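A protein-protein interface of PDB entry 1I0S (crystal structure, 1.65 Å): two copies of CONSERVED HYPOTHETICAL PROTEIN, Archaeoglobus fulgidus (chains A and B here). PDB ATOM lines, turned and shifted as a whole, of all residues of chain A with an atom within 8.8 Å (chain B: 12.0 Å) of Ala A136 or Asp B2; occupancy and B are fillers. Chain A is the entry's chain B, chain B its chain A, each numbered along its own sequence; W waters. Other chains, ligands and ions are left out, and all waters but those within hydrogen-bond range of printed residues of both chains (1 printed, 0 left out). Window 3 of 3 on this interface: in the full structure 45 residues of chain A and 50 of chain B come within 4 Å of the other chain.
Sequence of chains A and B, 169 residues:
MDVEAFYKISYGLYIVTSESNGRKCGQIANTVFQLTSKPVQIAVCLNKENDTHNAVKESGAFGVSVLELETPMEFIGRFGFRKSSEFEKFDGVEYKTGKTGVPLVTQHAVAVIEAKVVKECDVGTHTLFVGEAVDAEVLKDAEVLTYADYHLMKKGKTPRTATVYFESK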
ATOM      1  N   VAL A  40     -35.938  -6.240 -16.682  1.00  0.00           N
ATOM      2  CA  VAL A  40     -35.410  -4.910 -16.935  1.00  0.00           C
ATOM      3  C   VAL A  40     -35.618  -4.522 -18.401  1.00  0.00           C
ATOM      4  O   VAL A  40     -35.207  -5.243 -19.330  1.00  0.00           O
ATOM      5  CB  VAL A  40     -33.897  -4.804 -16.601  1.00  0.00           C
ATOM      6  CG1 VAL A  40     -33.372  -3.411 -16.997  1.00  0.00           C
ATOM      7  CG2 VAL A  40     -33.678  -5.015 -15.107  1.00  0.00           C
ATOM      8  N   ILE A  42     -35.307  -1.089 -21.037  1.00  0.00           N
ATOM      9  CA  ILE A  42     -34.742   0.245 -21.221  1.00  0.00           C
ATOM     10  C   ILE A  42     -35.338   0.840 -22.481  1.00  0.00           C
ATOM     11  O   ILE A  42     -35.456   0.160 -23.500  1.00  0.00           O
ATOM     12  CB  ILE A  42     -33.208   0.164 -21.431  1.00  0.00           C
ATOM     13  CG1 ILE A  42     -32.558  -0.561 -20.254  1.00  0.00           C
ATOM     14  CG2 ILE A  42     -32.635   1.548 -21.637  1.00  0.00           C
ATOM     15  CD1 ILE A  42     -32.689   0.163 -18.934  1.00  0.00           C
ATOM     16  N   VAL A  64     -26.112   0.909 -25.143  1.00  0.00           N
ATOM     17  CA  VAL A  64     -26.115   2.219 -24.505  1.00  0.00           C
ATOM     18  C   VAL A  64     -24.830   2.394 -23.706  1.00  0.00           C
ATOM     19  O   VAL A  64     -24.506   1.551 -22.872  1.00  0.00           O
ATOM     20  CB  VAL A  64     -27.311   2.362 -23.524  1.00  0.00           C
ATOM     21  CG1 VAL A  64     -27.245   3.713 -22.784  1.00  0.00           C
ATOM     22  CG2 VAL A  64     -28.629   2.223 -24.276  1.00  0.00           C
ATOM     23  N   LYS A  96     -16.366  -3.205 -27.747  1.00  0.00           N
ATOM     24  CA  LYS A  96     -16.374  -4.661 -27.858  1.00  0.00           C
ATOM     25  C   LYS A  96     -17.753  -4.992 -28.380  1.00  0.00           C
ATOM     26  O   LYS A  96     -18.656  -4.147 -28.322  1.00  0.00           O
ATOM     27  CB  LYS A  96     -16.141  -5.335 -26.505  1.00  0.00           C
ATOM     28  CG  LYS A  96     -17.180  -5.001 -25.443  1.00  0.00           C
ATOM     29  CD  LYS A  96     -16.747  -5.538 -24.113  1.00  0.00           C
ATOM     30  CE  LYS A  96     -17.701  -5.201 -22.993  1.00  0.00           C
ATOM     31  NZ  LYS A  96     -17.159  -5.734 -21.700  1.00  0.00           N
ATOM     32  N   LEU A 104     -20.514  -2.243 -28.245  1.00  0.00           N
ATOM     33  CA  LEU A 104     -20.661  -1.583 -26.956  1.00  0.00           C
ATOM     34  C   LEU A 104     -19.449  -0.682 -26.762  1.00  0.00           C
ATOM     35  O   LEU A 104     -18.346  -1.172 -26.518  1.00  0.00           O
ATOM     36  CB  LEU A 104     -20.748  -2.639 -25.851  1.00  0.00           C
ATOM     37  CG  LEU A 104     -21.993  -3.526 -26.003  1.00  0.00           C
ATOM     38  CD1 LEU A 104     -21.870  -4.773 -25.119  1.00  0.00           C
ATOM     39  CD2 LEU A 104     -23.245  -2.732 -25.637  1.00  0.00           C
ATOM     40  N   VAL A 110     -19.115   4.995 -18.140  1.00  0.00           N
ATOM     41  CA  VAL A 110     -19.179   4.583 -16.743  1.00  0.00           C
ATOM     42  C   VAL A 110     -19.834   3.200 -16.723  1.00  0.00           C
ATOM     43  O   VAL A 110     -19.558   2.368 -15.847  1.00  0.00           O
ATOM     44  CB  VAL A 110     -20.009   5.582 -15.909  1.00  0.00           C
ATOM     45  CG1 VAL A 110     -20.172   5.075 -14.480  1.00  0.00           C
ATOM     46  CG2 VAL A 110     -19.324   6.946 -15.909  1.00  0.00           C
ATOM     47  N   ALA A 111     -20.687   2.944 -17.713  1.00  0.00           N
ATOM     48  CA  ALA A 111     -21.367   1.664 -17.831  1.00  0.00           C
ATOM     49  C   ALA A 111     -21.885   1.457 -19.250  1.00  0.00           C
ATOM     50  O   ALA A 111     -21.978   2.405 -20.022  1.00  0.00           O
ATOM     51  CB  ALA A 111     -22.543   1.588 -16.844  1.00  0.00           C
ATOM     52  N   VAL A 112     -22.174   0.203 -19.588  1.00  0.00           N
ATOM     53  CA  VAL A 112     -22.742  -0.134 -20.891  1.00  0.00           C
ATOM     54  C   VAL A 112     -23.908  -1.080 -20.678  1.00  0.00           C
ATOM     55  O   VAL A 112     -23.911  -1.891 -19.740  1.00  0.00           O
ATOM     56  CB  VAL A 112     -21.714  -0.791 -21.862  1.00  0.00           C
ATOM     57  CG1 VAL A 112     -20.710   0.252 -22.333  1.00  0.00           C
ATOM     58  CG2 VAL A 112     -20.992  -1.961 -21.181  1.00  0.00           C
ATOM     59  N   ILE A 113     -24.911  -0.961 -21.539  1.00  0.00           N
ATOM     60  CA  ILE A 113     -26.103  -1.791 -21.469  1.00  0.00           C
ATOM     61  C   ILE A 113     -26.380  -2.312 -22.867  1.00  0.00           C
ATOM     62  O   ILE A 113     -26.275  -1.572 -23.840  1.00  0.00           O
ATOM     63  CB  ILE A 113     -27.341  -0.960 -21.022  1.00  0.00           C
ATOM     64  CG1 ILE A 113     -27.087  -0.381 -19.622  1.00  0.00           C
ATOM     65  CG2 ILE A 113     -28.598  -1.831 -21.046  1.00  0.00           C
ATOM     66  CD1 ILE A 113     -28.034   0.775 -19.206  1.00  0.00           C
ATOM     67  N   GLU A 114     -26.744  -3.585 -22.965  1.00  0.00           N
ATOM     68  CA  GLU A 114     -27.047  -4.189 -24.247  1.00  0.00           C
ATOM     69  C   GLU A 114     -28.493  -4.637 -24.193  1.00  0.00           C
ATOM     70  O   GLU A 114     -28.904  -5.257 -23.216  1.00  0.00           O
ATOM     71  CB  GLU A 114     -26.106  -5.375 -24.464  1.00  0.00           C
ATOM     72  CG  GLU A 114     -26.392  -6.194 -25.674  1.00  0.00           C
ATOM     73  CD  GLU A 114     -25.330  -7.272 -25.883  1.00  0.00           C
ATOM     74  OE1 GLU A 114     -24.735  -7.726 -24.882  1.00  0.00           O
ATOM     75  OE2 GLU A 114     -25.116  -7.655 -27.043  1.00  0.00           O
ATOM     76  N   ALA A 115     -29.274  -4.338 -25.232  1.00  0.00           N
ATOM     77  CA  ALA A 115     -30.686  -4.732 -25.226  1.00  0.00           C
ATOM     78  C   ALA A 115     -31.254  -5.233 -26.553  1.00  0.00           C
ATOM     79  O   ALA A 115     -30.767  -4.879 -27.626  1.00  0.00           O
ATOM     80  CB  ALA A 115     -31.541  -3.564 -24.722  1.00  0.00           C
ATOM     81  N   ALA A 133     -33.167  -5.604 -21.476  1.00  0.00           N
ATOM     82  CA  ALA A 133     -31.721  -5.660 -21.246  1.00  0.00           C
ATOM     83  C   ALA A 133     -31.260  -7.113 -21.203  1.00  0.00           C
ATOM     84  O   ALA A 133     -31.868  -7.934 -20.515  1.00  0.00           O
ATOM     85  CB  ALA A 133     -31.360  -4.956 -19.935  1.00  0.00           C
ATOM     86  N   VAL A 134     -30.203  -7.426 -21.947  1.00  0.00           N
ATOM     87  CA  VAL A 134     -29.661  -8.787 -21.962  1.00  0.00           C
ATOM     88  C   VAL A 134     -28.312  -8.839 -21.229  1.00  0.00           C
ATOM     89  O   VAL A 134     -27.896  -9.905 -20.757  1.00  0.00           O
ATOM     90  CB  VAL A 134     -29.526  -9.325 -23.401  1.00  0.00           C
ATOM     91  CG1 VAL A 134     -30.908  -9.534 -23.994  1.00  0.00           C
ATOM     92  CG2 VAL A 134     -28.717  -8.377 -24.254  1.00  0.00           C
ATOM     93  N   ASP A 135     -27.625  -7.702 -21.156  1.00  0.00           N
ATOM     94  CA  ASP A 135     -26.373  -7.589 -20.410  1.00  0.00           C
ATOM     95  C   ASP A 135     -26.206  -6.142 -19.973  1.00  0.00           C
ATOM     96  O   ASP A 135     -26.826  -5.236 -20.534  1.00  0.00           O
ATOM     97  CB  ASP A 135     -25.149  -8.004 -21.243  1.00  0.00           C
ATOM     98  CG  ASP A 135     -23.967  -8.432 -20.369  1.00  0.00           C
ATOM     99  OD1 ASP A 135     -22.892  -8.757 -20.932  1.00  0.00           O
ATOM    100  OD2 ASP A 135     -24.111  -8.458 -19.122  1.00  0.00           O
ATOM    101  N   ALA A 136     -25.376  -5.933 -18.960  1.00  0.00           N
ATOM    102  CA  ALA A 136     -25.093  -4.603 -18.448  1.00  0.00           C
ATOM    103  C   ALA A 136     -23.864  -4.757 -17.582  1.00  0.00           C
ATOM    104  O   ALA A 136     -23.705  -5.783 -16.914  1.00  0.00           O
ATOM    105  CB  ALA A 136     -26.282  -4.074 -17.620  1.00  0.00           C
ATOM    106  N   GLU A 137     -23.010  -3.743 -17.594  1.00  0.00           N
ATOM    107  CA  GLU A 137     -21.769  -3.776 -16.841  1.00  0.00           C
ATOM    108  C   GLU A 137     -21.319  -2.389 -16.398  1.00  0.00           C
ATOM    109  O   GLU A 137     -21.443  -1.416 -17.150  1.00  0.00           O
ATOM    110  CB  GLU A 137     -20.707  -4.440 -17.735  1.00  0.00           C
ATOM    111  CG  GLU A 137     -19.258  -4.196 -17.381  1.00  0.00           C
ATOM    112  CD  GLU A 137     -18.337  -4.989 -18.296  1.00  0.00           C
ATOM    113  OE1 GLU A 137     -18.750  -5.265 -19.446  1.00  0.00           O
ATOM    114  OE2 GLU A 137     -17.211  -5.328 -17.868  1.00  0.00           O
ATOM    115  N   VAL A 138     -20.831  -2.289 -15.166  1.00  0.00           N
ATOM    116  CA  VAL A 138     -20.305  -1.032 -14.660  1.00  0.00           C
ATOM    117  C   VAL A 138     -18.820  -1.107 -15.020  1.00  0.00           C
ATOM    118  O   VAL A 138     -18.163  -2.104 -14.718  1.00  0.00           O
ATOM    119  CB  VAL A 138     -20.503  -0.910 -13.139  1.00  0.00           C
ATOM    120  CG1 VAL A 138     -19.807   0.338 -12.618  1.00  0.00           C
ATOM    121  CG2 VAL A 138     -21.998  -0.830 -12.830  1.00  0.00           C
ATOM    122  N   LEU A 139     -18.300  -0.068 -15.668  1.00  0.00           N
ATOM    123  CA  LEU A 139     -16.911  -0.060 -16.140  1.00  0.00           C
ATOM    124  C   LEU A 139     -15.924   0.831 -15.406  1.00  0.00           C
ATOM    125  O   LEU A 139     -14.723   0.518 -15.340  1.00  0.00           O
ATOM    126  CB  LEU A 139     -16.879   0.357 -17.605  1.00  0.00           C
ATOM    127  CG  LEU A 139     -17.752  -0.381 -18.609  1.00  0.00           C
ATOM    128  CD1 LEU A 139     -17.795   0.424 -19.894  1.00  0.00           C
ATOM    129  CD2 LEU A 139     -17.218  -1.781 -18.845  1.00  0.00           C
ATOM    130  N   MET B   1     -25.545 -10.205 -15.751  1.00  0.00           N
ATOM    131  CA  MET B   1     -25.967  -8.783 -15.893  1.00  0.00           C
ATOM    132  C   MET B   1     -25.970  -8.112 -14.531  1.00  0.00           C
ATOM    133  O   MET B   1     -26.630  -8.577 -13.602  1.00  0.00           O
ATOM    134  CB  MET B   1     -27.357  -8.708 -16.510  1.00  0.00           C
ATOM    135  CG  MET B   1     -27.827  -7.287 -16.762  1.00  0.00           C
ATOM    136  SD  MET B   1     -29.249  -7.220 -17.861  1.00  0.00           S
ATOM    137  CE  MET B   1     -30.530  -7.712 -16.774  1.00  0.00           C
ATOM    138  N   ASP B   2     -25.233  -7.011 -14.437  1.00  0.00           N
ATOM    139  CA  ASP B   2     -25.088  -6.254 -13.204  1.00  0.00           C
ATOM    140  C   ASP B   2     -26.144  -5.163 -13.128  1.00  0.00           C
ATOM    141  O   ASP B   2     -26.023  -4.143 -13.799  1.00  0.00           O
ATOM    142  CB  ASP B   2     -23.701  -5.623 -13.160  1.00  0.00           C
ATOM    143  CG  ASP B   2     -23.431  -4.896 -11.861  1.00  0.00           C
ATOM    144  OD1 ASP B   2     -22.317  -4.363 -11.724  1.00  0.00           O
ATOM    145  OD2 ASP B   2     -24.327  -4.857 -10.980  1.00  0.00           O
ATOM    146  N   VAL B   3     -27.167  -5.378 -12.304  1.00  0.00           N
ATOM    147  CA  VAL B   3     -28.255  -4.408 -12.176  1.00  0.00           C
ATOM    148  C   VAL B   3     -27.808  -3.037 -11.713  1.00  0.00           C
ATOM    149  O   VAL B   3     -28.521  -2.055 -11.910  1.00  0.00           O
ATOM    150  CB  VAL B   3     -29.370  -4.910 -11.220  1.00  0.00           C
ATOM    151  CG1 VAL B   3     -29.998  -6.180 -11.783  1.00  0.00           C
ATOM    152  CG2 VAL B   3     -28.809  -5.134  -9.824  1.00  0.00           C
ATOM    153  N   GLU B   4     -26.625  -2.949 -11.117  1.00  0.00           N
ATOM    154  CA  GLU B   4     -26.137  -1.663 -10.666  1.00  0.00           C
ATOM    155  C   GLU B   4     -25.781  -0.740 -11.835  1.00  0.00           C
ATOM    156  O   GLU B   4     -25.621   0.463 -11.656  1.00  0.00           O
ATOM    157  CB  GLU B   4     -24.945  -1.863  -9.725  1.00  0.00           C
ATOM    158  CG  GLU B   4     -25.373  -2.522  -8.420  1.00  0.00           C
ATOM    159  CD  GLU B   4     -24.273  -2.602  -7.377  1.00  0.00           C
ATOM    160  OE1 GLU B   4     -24.600  -2.945  -6.219  1.00  0.00           O
ATOM    161  OE2 GLU B   4     -23.098  -2.329  -7.710  1.00  0.00           O
ATOM    162  N   ALA B   5     -25.665  -1.299 -13.036  1.00  0.00           N
ATOM    163  CA  ALA B   5     -25.346  -0.470 -14.200  1.00  0.00           C
ATOM    164  C   ALA B   5     -26.532   0.457 -14.468  1.00  0.00           C
ATOM    165  O   ALA B   5     -26.365   1.569 -14.974  1.00  0.00           O
ATOM    166  CB  ALA B   5     -25.097  -1.341 -15.422  1.00  0.00           C
ATOM    167  N   PHE B   6     -27.732   0.002 -14.128  1.00  0.00           N
ATOM    168  CA  PHE B   6     -28.905   0.833 -14.386  1.00  0.00           C
ATOM    169  C   PHE B   6     -28.987   2.031 -13.453  1.00  0.00           C
ATOM    170  O   PHE B   6     -29.707   2.985 -13.733  1.00  0.00           O
ATOM    171  CB  PHE B   6     -30.181  -0.018 -14.333  1.00  0.00           C
ATOM    172  CG  PHE B   6     -30.116  -1.245 -15.227  1.00  0.00           C
ATOM    173  CD1 PHE B   6     -30.041  -2.519 -14.680  1.00  0.00           C
ATOM    174  CD2 PHE B   6     -30.047  -1.114 -16.619  1.00  0.00           C
ATOM    175  CE1 PHE B   6     -29.890  -3.653 -15.500  1.00  0.00           C
ATOM    176  CE2 PHE B   6     -29.897  -2.249 -17.442  1.00  0.00           C
ATOM    177  CZ  PHE B   6     -29.817  -3.507 -16.876  1.00  0.00           C
ATOM    178  N   TYR B   7     -28.226   2.002 -12.364  1.00  0.00           N
ATOM    179  CA  TYR B   7     -28.182   3.124 -11.423  1.00  0.00           C
ATOM    180  C   TYR B   7     -27.494   4.326 -12.079  1.00  0.00           C
ATOM    181  O   TYR B   7     -27.658   5.459 -11.639  1.00  0.00           O
ATOM    182  CB  TYR B   7     -27.359   2.775 -10.172  1.00  0.00           C
ATOM    183  CG  TYR B   7     -27.821   1.594  -9.323  1.00  0.00           C
ATOM    184  CD1 TYR B   7     -27.039   1.155  -8.258  1.00  0.00           C
ATOM    185  CD2 TYR B   7     -29.024   0.945  -9.564  1.00  0.00           C
ATOM    186  CE1 TYR B   7     -27.445   0.084  -7.450  1.00  0.00           C
ATOM    187  CE2 TYR B   7     -29.447  -0.123  -8.761  1.00  0.00           C
ATOM    188  CZ  TYR B   7     -28.647  -0.548  -7.708  1.00  0.00           C
ATOM    189  OH  TYR B   7     -29.038  -1.623  -6.922  1.00  0.00           O
ATOM    190  N   LYS B   8     -26.728   4.065 -13.138  1.00  0.00           N
ATOM    191  CA  LYS B   8     -25.984   5.106 -13.815  1.00  0.00           C
ATOM    192  C   LYS B   8     -26.828   5.957 -14.758  1.00  0.00           C
ATOM    193  O   LYS B   8     -26.364   6.981 -15.228  1.00  0.00           O
ATOM    194  CB  LYS B   8     -24.793   4.495 -14.568  1.00  0.00           C
ATOM    195  CG  LYS B   8     -23.867   3.659 -13.661  1.00  0.00           C
ATOM    196  CD  LYS B   8     -23.351   4.455 -12.465  1.00  0.00           C
ATOM    197  CE  LYS B   8     -22.276   3.669 -11.673  1.00  0.00           C
ATOM    198  NZ  LYS B   8     -21.729   4.474 -10.533  1.00  0.00           N
ATOM    199  N   ILE B   9     -28.046   5.508 -15.051  1.00  0.00           N
ATOM    200  CA  ILE B   9     -28.975   6.278 -15.890  1.00  0.00           C
ATOM    201  C   ILE B   9     -29.485   7.460 -15.049  1.00  0.00           C
ATOM    202  O   ILE B   9     -29.877   7.279 -13.894  1.00  0.00           O
ATOM    203  CB  ILE B   9     -30.161   5.399 -16.319  1.00  0.00           C
ATOM    204  CG1 ILE B   9     -29.661   4.249 -17.204  1.00  0.00           C
ATOM    205  CG2 ILE B   9     -31.218   6.241 -17.044  1.00  0.00           C
ATOM    206  CD1 ILE B   9     -30.735   3.233 -17.540  1.00  0.00           C
ATOM    207  N   TYR B  11     -31.993  10.731 -14.011  1.00  0.00           N
ATOM    208  CA  TYR B  11     -33.422  11.099 -14.008  1.00  0.00           C
ATOM    209  C   TYR B  11     -33.633  12.334 -13.149  1.00  0.00           C
ATOM    210  O   TYR B  11     -32.780  12.726 -12.337  1.00  0.00           O
ATOM    211  CB  TYR B  11     -34.319  10.031 -13.351  1.00  0.00           C
ATOM    212  CG  TYR B  11     -34.215   8.634 -13.868  1.00  0.00           C
ATOM    213  CD1 TYR B  11     -33.126   7.823 -13.539  1.00  0.00           C
ATOM    214  CD2 TYR B  11     -35.206   8.114 -14.696  1.00  0.00           C
ATOM    215  CE1 TYR B  11     -33.033   6.525 -14.033  1.00  0.00           C
ATOM    216  CE2 TYR B  11     -35.120   6.819 -15.199  1.00  0.00           C
ATOM    217  CZ  TYR B  11     -34.027   6.037 -14.862  1.00  0.00           C
ATOM    218  OH  TYR B  11     -33.914   4.766 -15.386  1.00  0.00           O
HETATM  219  O   HOH W   1     -20.432  -4.723 -13.679  1.00  0.00           O
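No position is printed for both chains.
The side-chain carboxylate of Asp B2 sits at hydrogen-bond distance from the backbone NH of Glu B4 (3.0 Å).
The backbone NH of Ala A133 is in hydrogen-bond range of the backbone carbonyl oxygen of Val A40.
The side-chain carboxylate (OE1) of Glu A137 lies within salt-bridge range of the side-chain amino group (NZ) of Lys A96, at 2.8 Å.
O of Val A112 sits at hydrogen-bond distance from N of Glu A137 (3.0 Å).
The backbone carbonyl oxygen (O) of Glu A114 lies within hydrogen-bond range of the backbone NH (N) of Val A134 (2.8 Å).
O of Asp A135 is in hydrogen-bond range of N of Glu A114, at 2.9 Å.
Among the printed residues, pairs that only touch across the chains: Val A40 with Phe B6, Ile A42 with Phe B6, Ile A42 with Ile B9, Val A110 with Lys B8, Ile A113 with Phe B6, Ala A133 with Phe B6, Val A134 with Met B1, Ala A136 with Met B1, Ala A136 with Ala B5, Ala A136 with Phe B6, Glu A137 with Ala B5, Val A138 with Asp B2, Val A138 with Glu B4 and Val A138 with Ala B5.
Of the 18 printed residues of chain A, 10 touch a printed residue of chain B.
Hydrophobic or aromatic side chains of chain A that line the printed part of chain B: Val A40, Ile A42, Val A110, Ile A113, Ala A133, Ala A136 and Val A138.
Of the 10 printed residues of chain B, 7 touch a printed residue of chain A.
Hydrophobic or aromatic side chains of chain B within 4 Å of the printed part of chain A: Met B1, Ala B5, Phe B6 and Ile B9.
Among the printed residues, 17 pairs touch across the chains.
The backbone NH of Asp A135 lies within hydrogen-bond range of the side-chain sulfur of Met B1, 3.7 Å away.
The backbone carbonyl oxygen (O) of Ala A136 is in hydrogen-bond range of the backbone NH (N) of Asp B2, 3.2 Å away.
The backbone carbonyl oxygen (O) of Ala A133 sits close to the side-chain sulfur (SD) of Met B1, at 3.8 Å.
Ala A111 touches none of the printed residues of chain B.
No residue of chain B comes within 4 Å of Val A112.
Of the printed residues of chain B, Val A134 touches Met B1.
Asp A135 touches one residue of chain B.
Ala A136 touches just these residues of chain B: Met B1, Asp B2, Ala B5 and Phe B6.
Of the printed residues of chain B, Glu A137 touches Ala B5.
Val A138 touches just these residues of chain B: Asp B2, Glu B4 and Ala B5.
Val B3 touches none of the printed residues of chain A.
Printed residues of chain A within 4 Å of Ala B5: Ala A136 (3.7 Å), Glu A137 (3.9 Å) and Val A138 (3.6 Å).
Tyr B11 touches none of the printed residues of chain A.
The nearest residue of chain B that does not touch Ala A136 is Val B3 (5.5 Å).
The nearest residue of chain A that does not touch Asp B2 is Glu A137 (4.5 Å).
Water W1 lies within hydrogen-bond range of the side-chain carboxylate of Asp B2 (2.7 Å) and the backbone NH of Val A138 (2.9 Å).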
